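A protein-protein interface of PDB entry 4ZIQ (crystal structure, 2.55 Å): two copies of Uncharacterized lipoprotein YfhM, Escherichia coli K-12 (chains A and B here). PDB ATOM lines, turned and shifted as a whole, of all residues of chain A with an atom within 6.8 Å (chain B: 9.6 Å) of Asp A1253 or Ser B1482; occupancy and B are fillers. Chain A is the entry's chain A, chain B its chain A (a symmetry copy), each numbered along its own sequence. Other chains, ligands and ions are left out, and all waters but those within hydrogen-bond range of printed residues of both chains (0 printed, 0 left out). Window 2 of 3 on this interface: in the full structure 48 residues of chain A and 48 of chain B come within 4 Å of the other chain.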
ATOM      1  N   LEU A1248     -10.982 -12.003  -3.653  1.00  0.00           N
ATOM      2  CA  LEU A1248     -11.410 -12.765  -2.484  1.00  0.00           C
ATOM      3  C   LEU A1248     -10.432 -12.540  -1.321  1.00  0.00           C
ATOM      4  O   LEU A1248     -10.889 -12.427  -0.188  1.00  0.00           O
ATOM      5  CB  LEU A1248     -11.558 -14.263  -2.817  1.00  0.00           C
ATOM      6  CG  LEU A1248     -12.067 -15.198  -1.682  1.00  0.00           C
ATOM      7  CD1 LEU A1248     -13.314 -14.638  -0.970  1.00  0.00           C
ATOM      8  CD2 LEU A1248     -12.326 -16.610  -2.202  1.00  0.00           C
ATOM      9  N   ARG A1249      -9.118 -12.394  -1.594  1.00  0.00           N
ATOM     10  CA  ARG A1249      -8.153 -12.058  -0.535  1.00  0.00           C
ATOM     11  C   ARG A1249      -8.445 -10.681   0.040  1.00  0.00           C
ATOM     12  O   ARG A1249      -8.254 -10.493   1.224  1.00  0.00           O
ATOM     13  CB  ARG A1249      -6.695 -12.121  -1.022  1.00  0.00           C
ATOM     14  CG  ARG A1249      -6.274 -13.530  -1.431  1.00  0.00           C
ATOM     15  CD  ARG A1249      -5.461 -14.240  -0.375  1.00  0.00           C
ATOM     16  NE  ARG A1249      -6.172 -14.475   0.885  1.00  0.00           N
ATOM     17  CZ  ARG A1249      -5.800 -13.972   2.060  1.00  0.00           C
ATOM     18  NH1 ARG A1249      -4.748 -13.162   2.142  1.00  0.00           N
ATOM     19  NH2 ARG A1249      -6.477 -14.273   3.160  1.00  0.00           N
ATOM     20  N   TYR A1250      -8.936  -9.734  -0.779  1.00  0.00           N
ATOM     21  CA  TYR A1250      -9.300  -8.388  -0.338  1.00  0.00           C
ATOM     22  C   TYR A1250     -10.490  -8.405   0.625  1.00  0.00           C
ATOM     23  O   TYR A1250     -10.550  -7.585   1.540  1.00  0.00           O
ATOM     24  CB  TYR A1250      -9.667  -7.492  -1.538  1.00  0.00           C
ATOM     25  CG  TYR A1250      -8.560  -7.121  -2.503  1.00  0.00           C
ATOM     26  CD1 TYR A1250      -7.261  -7.596  -2.328  1.00  0.00           C
ATOM     27  CD2 TYR A1250      -8.822  -6.332  -3.619  1.00  0.00           C
ATOM     28  CE1 TYR A1250      -6.249  -7.279  -3.233  1.00  0.00           C
ATOM     29  CE2 TYR A1250      -7.817  -6.004  -4.525  1.00  0.00           C
ATOM     30  CZ  TYR A1250      -6.528  -6.467  -4.319  1.00  0.00           C
ATOM     31  OH  TYR A1250      -5.533  -6.100  -5.185  1.00  0.00           O
ATOM     32  N   LEU A1251     -11.468  -9.288   0.388  1.00  0.00           N
ATOM     33  CA  LEU A1251     -12.639  -9.364   1.260  1.00  0.00           C
ATOM     34  C   LEU A1251     -12.279  -9.973   2.600  1.00  0.00           C
ATOM     35  O   LEU A1251     -12.760  -9.513   3.632  1.00  0.00           O
ATOM     36  CB  LEU A1251     -13.783 -10.186   0.625  1.00  0.00           C
ATOM     37  CG  LEU A1251     -14.306  -9.845  -0.781  1.00  0.00           C
ATOM     38  CD1 LEU A1251     -15.524 -10.697  -1.105  1.00  0.00           C
ATOM     39  CD2 LEU A1251     -14.664  -8.379  -0.910  1.00  0.00           C
ATOM     40  N   GLN A1252     -11.434 -11.010   2.574  1.00  0.00           N
ATOM     41  CA  GLN A1252     -11.020 -11.808   3.730  1.00  0.00           C
ATOM     42  C   GLN A1252      -9.890 -11.186   4.535  1.00  0.00           C
ATOM     43  O   GLN A1252      -9.844 -11.329   5.766  1.00  0.00           O
ATOM     44  CB  GLN A1252     -10.554 -13.202   3.255  1.00  0.00           C
ATOM     45  CG  GLN A1252     -11.635 -14.042   2.560  1.00  0.00           C
ATOM     46  CD  GLN A1252     -11.120 -15.316   1.927  1.00  0.00           C
ATOM     47  OE1 GLN A1252      -9.929 -15.479   1.620  1.00  0.00           O
ATOM     48  NE2 GLN A1252     -12.028 -16.250   1.704  1.00  0.00           N
ATOM     49  N   ASP A1253      -8.941 -10.552   3.841  1.00  0.00           N
ATOM     50  CA  ASP A1253      -7.737 -10.036   4.473  1.00  0.00           C
ATOM     51  C   ASP A1253      -7.472  -8.532   4.204  1.00  0.00           C
ATOM     52  O   ASP A1253      -6.446  -8.213   3.605  1.00  0.00           O
ATOM     53  CB  ASP A1253      -6.543 -10.888   3.996  1.00  0.00           C
ATOM     54  CG  ASP A1253      -5.387 -10.991   4.957  1.00  0.00           C
ATOM     55  OD1 ASP A1253      -5.327 -10.177   5.905  1.00  0.00           O
ATOM     56  OD2 ASP A1253      -4.505 -11.845   4.730  1.00  0.00           O
ATOM     57  N   PRO A1254      -8.291  -7.574   4.707  1.00  0.00           N
ATOM     58  CA  PRO A1254      -7.929  -6.142   4.526  1.00  0.00           C
ATOM     59  C   PRO A1254      -6.625  -5.755   5.253  1.00  0.00           C
ATOM     60  O   PRO A1254      -5.982  -4.778   4.887  1.00  0.00           O
ATOM     61  CB  PRO A1254      -9.115  -5.386   5.149  1.00  0.00           C
ATOM     62  CG  PRO A1254      -9.750  -6.363   6.085  1.00  0.00           C
ATOM     63  CD  PRO A1254      -9.547  -7.722   5.477  1.00  0.00           C
ATOM     64  N   GLY A1255      -6.260  -6.523   6.279  1.00  0.00           N
ATOM     65  CA  GLY A1255      -5.081  -6.294   7.103  1.00  0.00           C
ATOM     66  C   GLY A1255      -3.753  -6.373   6.383  1.00  0.00           C
ATOM     67  O   GLY A1255      -2.786  -5.758   6.823  1.00  0.00           O
ATOM     68  N   MET A1256      -3.672  -7.115   5.274  1.00  0.00           N
ATOM     69  CA  MET A1256      -2.391  -7.206   4.565  1.00  0.00           C
ATOM     70  C   MET A1256      -2.209  -6.056   3.540  1.00  0.00           C
ATOM     71  O   MET A1256      -1.186  -6.013   2.860  1.00  0.00           O
ATOM     72  CB  MET A1256      -2.212  -8.592   3.898  1.00  0.00           C
ATOM     73  CG  MET A1256      -3.341  -9.018   2.992  1.00  0.00           C
ATOM     74  SD  MET A1256      -3.485  -8.217   1.368  1.00  0.00           S
ATOM     75  CE  MET A1256      -1.883  -8.590   0.705  1.00  0.00           C
ATOM     76  N   MET A1257      -3.187  -5.140   3.433  1.00  0.00           N
ATOM     77  CA  MET A1257      -3.138  -4.031   2.479  1.00  0.00           C
ATOM     78  C   MET A1257      -2.194  -2.916   2.947  1.00  0.00           C
ATOM     79  O   MET A1257      -2.379  -2.340   4.028  1.00  0.00           O
ATOM     80  CB  MET A1257      -4.543  -3.458   2.196  1.00  0.00           C
ATOM     81  CG  MET A1257      -5.420  -4.362   1.362  1.00  0.00           C
ATOM     82  SD  MET A1257      -7.059  -3.644   1.014  1.00  0.00           S
ATOM     83  CE  MET A1257      -7.969  -5.096   0.772  1.00  0.00           C
ATOM     84  N   GLN A1273     -12.494  -3.061  -0.634  1.00  0.00           N
ATOM     85  CA  GLN A1273     -13.284  -4.249  -0.329  1.00  0.00           C
ATOM     86  C   GLN A1273     -14.677  -4.202  -0.956  1.00  0.00           C
ATOM     87  O   GLN A1273     -15.140  -5.215  -1.484  1.00  0.00           O
ATOM     88  CB  GLN A1273     -13.400  -4.470   1.185  1.00  0.00           C
ATOM     89  CG  GLN A1273     -12.068  -4.751   1.915  1.00  0.00           C
ATOM     90  CD  GLN A1273     -12.335  -5.216   3.325  1.00  0.00           C
ATOM     91  OE1 GLN A1273     -12.745  -4.433   4.185  1.00  0.00           O
ATOM     92  NE2 GLN A1273     -12.200  -6.516   3.581  1.00  0.00           N
ATOM     93  N   ARG B1473       1.499  -1.762  13.961  1.00  0.00           N
ATOM     94  CA  ARG B1473       2.130  -3.069  13.807  1.00  0.00           C
ATOM     95  C   ARG B1473       1.141  -4.086  13.262  1.00  0.00           C
ATOM     96  O   ARG B1473      -0.041  -4.102  13.631  1.00  0.00           O
ATOM     97  CB  ARG B1473       2.695  -3.553  15.148  1.00  0.00           C
ATOM     98  CG  ARG B1473       3.639  -4.722  15.003  1.00  0.00           C
ATOM     99  CD  ARG B1473       3.604  -5.631  16.205  1.00  0.00           C
ATOM    100  NE  ARG B1473       4.348  -5.072  17.324  1.00  0.00           N
ATOM    101  CZ  ARG B1473       3.837  -4.874  18.533  1.00  0.00           C
ATOM    102  NH1 ARG B1473       2.574  -5.196  18.790  1.00  0.00           N
ATOM    103  NH2 ARG B1473       4.591  -4.377  19.504  1.00  0.00           N
ATOM    104  N   HIS B1474       1.641  -4.957  12.402  1.00  0.00           N
ATOM    105  CA  HIS B1474       0.875  -6.059  11.835  1.00  0.00           C
ATOM    106  C   HIS B1474       1.801  -7.212  11.630  1.00  0.00           C
ATOM    107  O   HIS B1474       2.949  -7.011  11.240  1.00  0.00           O
ATOM    108  CB  HIS B1474       0.186  -5.659  10.528  1.00  0.00           C
ATOM    109  CG  HIS B1474      -0.903  -6.599  10.152  1.00  0.00           C
ATOM    110  ND1 HIS B1474      -2.130  -6.572  10.792  1.00  0.00           N
ATOM    111  CD2 HIS B1474      -0.907  -7.595   9.239  1.00  0.00           C
ATOM    112  CE1 HIS B1474      -2.850  -7.532  10.226  1.00  0.00           C
ATOM    113  NE2 HIS B1474      -2.148  -8.179   9.297  1.00  0.00           N
ATOM    114  N   ILE B1475       1.312  -8.418  11.901  1.00  0.00           N
ATOM    115  CA  ILE B1475       2.072  -9.652  11.761  1.00  0.00           C
ATOM    116  C   ILE B1475       1.483 -10.484  10.603  1.00  0.00           C
ATOM    117  O   ILE B1475       0.287 -10.793  10.545  1.00  0.00           O
ATOM    118  CB  ILE B1475       2.163 -10.434  13.105  1.00  0.00           C
ATOM    119  CG1 ILE B1475       2.871  -9.553  14.188  1.00  0.00           C
ATOM    120  CG2 ILE B1475       2.903 -11.751  12.923  1.00  0.00           C
ATOM    121  CD1 ILE B1475       2.759 -10.049  15.620  1.00  0.00           C
ATOM    122  N   LEU B1476       2.366 -10.790   9.657  1.00  0.00           N
ATOM    123  CA  LEU B1476       2.081 -11.598   8.493  1.00  0.00           C
ATOM    124  C   LEU B1476       2.860 -12.877   8.581  1.00  0.00           C
ATOM    125  O   LEU B1476       3.893 -12.933   9.264  1.00  0.00           O
ATOM    126  CB  LEU B1476       2.466 -10.843   7.207  1.00  0.00           C
ATOM    127  CG  LEU B1476       1.910  -9.431   7.004  1.00  0.00           C
ATOM    128  CD1 LEU B1476       2.737  -8.701   6.025  1.00  0.00           C
ATOM    129  CD2 LEU B1476       0.464  -9.458   6.521  1.00  0.00           C
ATOM    130  N   GLY B1477       2.338 -13.905   7.922  1.00  0.00           N
ATOM    131  CA  GLY B1477       3.013 -15.180   7.778  1.00  0.00           C
ATOM    132  C   GLY B1477       3.945 -15.026   6.587  1.00  0.00           C
ATOM    133  O   GLY B1477       3.826 -14.060   5.813  1.00  0.00           O
ATOM    134  N   THR B1478       4.869 -15.976   6.402  1.00  0.00           N
ATOM    135  CA  THR B1478       5.811 -15.918   5.284  1.00  0.00           C
ATOM    136  C   THR B1478       5.076 -16.150   3.935  1.00  0.00           C
ATOM    137  O   THR B1478       5.685 -15.979   2.880  1.00  0.00           O
ATOM    138  CB  THR B1478       7.008 -16.845   5.513  1.00  0.00           C
ATOM    139  OG1 THR B1478       6.537 -18.166   5.773  1.00  0.00           O
ATOM    140  CG2 THR B1478       7.910 -16.358   6.673  1.00  0.00           C
ATOM    141  N   ASP B1479       3.755 -16.411   3.975  1.00  0.00           N
ATOM    142  CA  ASP B1479       2.917 -16.560   2.781  1.00  0.00           C
ATOM    143  C   ASP B1479       2.293 -15.213   2.359  1.00  0.00           C
ATOM    144  O   ASP B1479       1.489 -15.179   1.428  1.00  0.00           O
ATOM    145  CB  ASP B1479       1.815 -17.625   3.001  1.00  0.00           C
ATOM    146  CG  ASP B1479       0.752 -17.367   4.072  1.00  0.00           C
ATOM    147  OD1 ASP B1479       0.920 -16.407   4.885  1.00  0.00           O
ATOM    148  OD2 ASP B1479      -0.228 -18.148   4.130  1.00  0.00           O
ATOM    149  N   GLY B1480       2.650 -14.133   3.056  1.00  0.00           N
ATOM    150  CA  GLY B1480       2.134 -12.791   2.787  1.00  0.00           C
ATOM    151  C   GLY B1480       0.730 -12.501   3.300  1.00  0.00           C
ATOM    152  O   GLY B1480       0.215 -11.404   3.093  1.00  0.00           O
ATOM    153  N   LYS B1481       0.087 -13.470   3.951  1.00  0.00           N
ATOM    154  CA  LYS B1481      -1.250 -13.286   4.526  1.00  0.00           C
ATOM    155  C   LYS B1481      -1.130 -12.897   5.979  1.00  0.00           C
ATOM    156  O   LYS B1481      -0.106 -13.214   6.595  1.00  0.00           O
ATOM    157  CB  LYS B1481      -2.083 -14.571   4.425  1.00  0.00           C
ATOM    158  CG  LYS B1481      -2.163 -15.178   3.046  1.00  0.00           C
ATOM    159  CD  LYS B1481      -3.129 -16.355   3.035  1.00  0.00           C
ATOM    160  CE  LYS B1481      -3.013 -17.243   1.815  1.00  0.00           C
ATOM    161  NZ  LYS B1481      -3.116 -16.483   0.544  1.00  0.00           N
ATOM    162  N   SER B1482      -2.163 -12.242   6.545  1.00  0.00           N
ATOM    163  CA  SER B1482      -2.182 -11.920   7.971  1.00  0.00           C
ATOM    164  C   SER B1482      -2.106 -13.213   8.780  1.00  0.00           C
ATOM    165  O   SER B1482      -2.820 -14.174   8.455  1.00  0.00           O
ATOM    166  CB  SER B1482      -3.444 -11.147   8.331  1.00  0.00           C
ATOM    167  OG  SER B1482      -3.428  -9.854   7.747  1.00  0.00           O
ATOM    168  N   LYS B1483      -1.186 -13.280   9.754  1.00  0.00           N
ATOM    169  CA  LYS B1483      -1.044 -14.469  10.591  1.00  0.00           C
ATOM    170  C   LYS B1483      -2.058 -14.429  11.732  1.00  0.00           C
ATOM    171  O   LYS B1483      -2.155 -13.434  12.451  1.00  0.00           O
ATOM    172  CB  LYS B1483       0.395 -14.608  11.150  1.00  0.00           C
ATOM    173  CG  LYS B1483       0.652 -15.931  11.913  1.00  0.00           C
ATOM    174  CD  LYS B1483       1.305 -17.002  11.043  1.00  0.00           C
ATOM    175  CE  LYS B1483       1.251 -18.382  11.663  1.00  0.00           C
ATOM    176  NZ  LYS B1483      -0.069 -19.048  11.467  1.00  0.00           N
ATOM    177  N   SER B1484      -2.796 -15.532  11.898  1.00  0.00           N
ATOM    178  CA  SER B1484      -3.761 -15.752  12.980  1.00  0.00           C
ATOM    179  C   SER B1484      -2.963 -16.040  14.271  1.00  0.00           C
ATOM    180  O   SER B1484      -2.449 -17.157  14.461  1.00  0.00           O
ATOM    181  CB  SER B1484      -4.716 -16.888  12.615  1.00  0.00           C
ATOM    182  OG  SER B1484      -4.201 -17.663  11.544  1.00  0.00           O
ATOM    183  N   LEU B1485      -2.823 -14.986  15.120  1.00  0.00           N
ATOM    184  CA  LEU B1485      -2.040 -14.906  16.370  1.00  0.00           C
ATOM    185  C   LEU B1485      -2.418 -15.926  17.479  1.00  0.00           C
ATOM    186  O   LEU B1485      -1.929 -15.814  18.616  1.00  0.00           O
ATOM    187  CB  LEU B1485      -2.132 -13.486  16.956  1.00  0.00           C
ATOM    188  CG  LEU B1485      -1.379 -12.379  16.221  1.00  0.00           C
ATOM    189  CD1 LEU B1485      -1.350 -11.099  17.053  1.00  0.00           C
ATOM    190  CD2 LEU B1485       0.051 -12.800  15.892  1.00  0.00           C
ATOM    191  N   ASP B1486      -3.271 -16.906  17.146  1.00  0.00           N
ATOM    192  CA  ASP B1486      -3.689 -17.977  18.036  1.00  0.00           C
ATOM    193  C   ASP B1486      -3.096 -19.269  17.503  1.00  0.00           C
ATOM    194  O   ASP B1486      -2.516 -20.047  18.269  1.00  0.00           O
ATOM    195  CB  ASP B1486      -5.227 -18.047  18.148  1.00  0.00           C
ATOM    196  CG  ASP B1486      -5.957 -18.052  16.817  1.00  0.00           C
ATOM    197  OD1 ASP B1486      -6.285 -19.157  16.321  1.00  0.00           O
ATOM    198  OD2 ASP B1486      -6.164 -16.954  16.252  1.00  0.00           O
ATOM    199  N   SER B1487      -3.178 -19.449  16.159  1.00  0.00           N
ATOM    200  CA  SER B1487      -2.679 -20.586  15.387  1.00  0.00           C
ATOM    201  C   SER B1487      -1.150 -20.481  15.156  1.00  0.00           C
ATOM    202  O   SER B1487      -0.643 -20.956  14.137  1.00  0.00           O
ATOM    203  CB  SER B1487      -3.428 -20.678  14.058  1.00  0.00           C
ATOM    204  OG  SER B1487      -3.218 -21.923  13.414  1.00  0.00           O
ATOM    205  N   LEU B1488      -0.419 -19.910  16.131  1.00  0.00           N
ATOM    206  CA  LEU B1488       1.037 -19.794  16.093  1.00  0.00           C
ATOM    207  C   LEU B1488       1.695 -21.013  16.783  1.00  0.00           C
ATOM    208  O   LEU B1488       1.331 -21.357  17.899  1.00  0.00           O
ATOM    209  CB  LEU B1488       1.461 -18.484  16.763  1.00  0.00           C
ATOM    210  CG  LEU B1488       2.830 -17.949  16.431  1.00  0.00           C
ATOM    211  CD1 LEU B1488       3.074 -17.886  14.936  1.00  0.00           C
ATOM    212  CD2 LEU B1488       2.995 -16.606  17.008  1.00  0.00           C
ATOM    213  N   VAL B1494       7.662 -15.579  11.359  1.00  0.00           N
ATOM    214  CA  VAL B1494       6.648 -14.562  11.082  1.00  0.00           C
ATOM    215  C   VAL B1494       7.356 -13.289  10.648  1.00  0.00           C
ATOM    216  O   VAL B1494       8.513 -13.072  11.003  1.00  0.00           O
ATOM    217  CB  VAL B1494       5.646 -14.294  12.251  1.00  0.00           C
ATOM    218  CG1 VAL B1494       4.811 -15.531  12.573  1.00  0.00           C
ATOM    219  CG2 VAL B1494       6.341 -13.739  13.502  1.00  0.00           C
ATOM    220  N   LEU B1495       6.648 -12.461   9.875  1.00  0.00           N
ATOM    221  CA  LEU B1495       7.118 -11.184   9.392  1.00  0.00           C
ATOM    222  C   LEU B1495       6.381 -10.112  10.131  1.00  0.00           C
ATOM    223  O   LEU B1495       5.164 -10.026  10.030  1.00  0.00           O
ATOM    224  CB  LEU B1495       6.933 -11.048   7.874  1.00  0.00           C
ATOM    225  CG  LEU B1495       7.755 -12.017   7.025  1.00  0.00           C
ATOM    226  CD1 LEU B1495       7.006 -12.392   5.738  1.00  0.00           C
ATOM    227  CD2 LEU B1495       9.119 -11.432   6.709  1.00  0.00           C
ATOM    228  N   TRP B1497       5.567  -6.384  10.574  1.00  0.00           N
ATOM    229  CA  TRP B1497       5.503  -5.193   9.756  1.00  0.00           C
ATOM    230  C   TRP B1497       5.101  -3.955  10.587  1.00  0.00           C
ATOM    231  O   TRP B1497       4.021  -3.905  11.188  1.00  0.00           O
ATOM    232  CB  TRP B1497       4.537  -5.475   8.595  1.00  0.00           C
ATOM    233  CG  TRP B1497       4.021  -4.293   7.828  1.00  0.00           C
ATOM    234  CD1 TRP B1497       4.665  -3.115   7.576  1.00  0.00           C
ATOM    235  CD2 TRP B1497       2.764  -4.221   7.138  1.00  0.00           C
ATOM    236  NE1 TRP B1497       3.859  -2.287   6.827  1.00  0.00           N
ATOM    237  CE2 TRP B1497       2.685  -2.941   6.546  1.00  0.00           C
ATOM    238  CE3 TRP B1497       1.668  -5.103   7.008  1.00  0.00           C
ATOM    239  CZ2 TRP B1497       1.574  -2.529   5.799  1.00  0.00           C
ATOM    240  CZ3 TRP B1497       0.563  -4.694   6.268  1.00  0.00           C
ATOM    241  CH2 TRP B1497       0.534  -3.436   5.650  1.00  0.00           C
ATOM    242  N   GLU B1539       7.159 -12.906  -0.325  1.00  0.00           N
ATOM    243  CA  GLU B1539       5.734 -12.613  -0.463  1.00  0.00           C
ATOM    244  C   GLU B1539       5.387 -11.205   0.024  1.00  0.00           C
ATOM    245  O   GLU B1539       4.247 -10.786  -0.172  1.00  0.00           O
ATOM    246  CB  GLU B1539       4.859 -13.663   0.255  1.00  0.00           C
ATOM    247  CG  GLU B1539       4.959 -15.070  -0.318  1.00  0.00           C
ATOM    248  CD  GLU B1539       4.727 -15.249  -1.811  1.00  0.00           C
ATOM    249  OE1 GLU B1539       3.825 -14.585  -2.376  1.00  0.00           O
ATOM    250  OE2 GLU B1539       5.450 -16.078  -2.410  1.00  0.00           O
ATOM    251  N   VAL B1540       6.353 -10.467   0.634  1.00  0.00           N
ATOM    252  CA  VAL B1540       6.165  -9.085   1.093  1.00  0.00           C
ATOM    253  C   VAL B1540       7.246  -8.189   0.458  1.00  0.00           C
ATOM    254  O   VAL B1540       7.701  -7.213   1.059  1.00  0.00           O
ATOM    255  CB  VAL B1540       6.101  -8.936   2.634  1.00  0.00           C
ATOM    256  CG1 VAL B1540       4.817  -9.524   3.192  1.00  0.00           C
ATOM    257  CG2 VAL B1540       7.331  -9.533   3.325  1.00  0.00           C
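The side-chain carboxylate (OD1) of Asp A1253 lies within hydrogen-bond range of the side-chain hydroxyl (OG) of Ser B1482 (2.7 Å).
The guanidinium group (NH1) of Arg A1249 lies within salt-bridge range of the side-chain carboxylate (OD2) of Asp A1253 (2.9 Å). The backbone carbonyl oxygen (O) of Leu B1476 sits at hydrogen-bond distance from the backbone NH (N) of Leu B1495. NE2 of His B1474 sits at hydrogen-bond distance from OG of Ser B1482 (2.6 Å). The backbone carbonyl oxygen (O) of His B1474 is in hydrogen-bond range of the backbone NH (N) of Trp B1497, at 2.8 Å. The side-chain carboxylate (OD1) of Asp B1479 sits at hydrogen-bond distance from the backbone NH (N) of Lys B1481 (3.2 Å).
Lys B1481 touches Arg A1249. Lys B1481 touches Asp A1253. Gly A1255 touches His B1474. Ser B1482 touches Gly A1255. O of Gly A1255 touches CZ3 of Trp B1497, at 3.6 Å. Leu B1476 touches Met A1256. CB of Met A1256 touches O of Gly B1480 (3.8 Å). OG of Ser B1482 touches N of Met A1256, at 3.7 Å. Met A1257 touches Trp B1497 (O to CH2, 3.5 Å).
Of chain B, only Lys B1481 (3.6 Å) and Ser B1482 (2.7 Å) come within 4 Å of Asp A1253. No residue of chain B comes within 4 Å of Pro A1254. Of the printed residues of chain B, Gly A1255 touches His B1474 (3.5 Å), Ser B1482 (3.8 Å) and Trp B1497 (3.6 Å). Of the printed residues of chain B, Met A1257 touches Trp B1497 (3.5 Å). Gln A1273 touches none of the printed residues of chain B. Printed residues of chain A within 4 Å of Leu B1476: Met A1256 (3.8 Å). Of the printed residues of chain A, Gly B1480 touches Met A1256. Printed residues of chain A within 4 Å of Lys B1481: Arg A1249 and Asp A1253. Of chain A, only Asp A1253 (2.7 Å), Gly A1255 (3.8 Å) and Met A1256 (3.7 Å) come within 4 Å of Ser B1482. Leu B1488 touches none of the printed residues of chain A. Of the printed residues of chain A, Trp B1497 touches Gly A1255 (3.6 Å) and Met A1257 (3.5 Å). The nearest residue of chain B that does not touch Asp A1253 is Gly B1480 (5.0 Å).
Printed residues of chain A that touch a printed residue of chain B: Arg A1249, Asp A1253, Gly A1255, Met A1256 and Met A1257. Along chain A the printed residues that touch a printed residue of chain B span positions 1249 to 1257. Of the 21 printed residues of chain B, 6 touch a printed residue of chain A. Among the printed residues, no Asp or Glu carboxylate lies within 4 Å of a Lys or Arg side-chain nitrogen of the other chain.
No position is printed for both chains. Of the 10 pairs that touch across the chains among the printed residues, none has its exchanged pair printed and touching as well.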
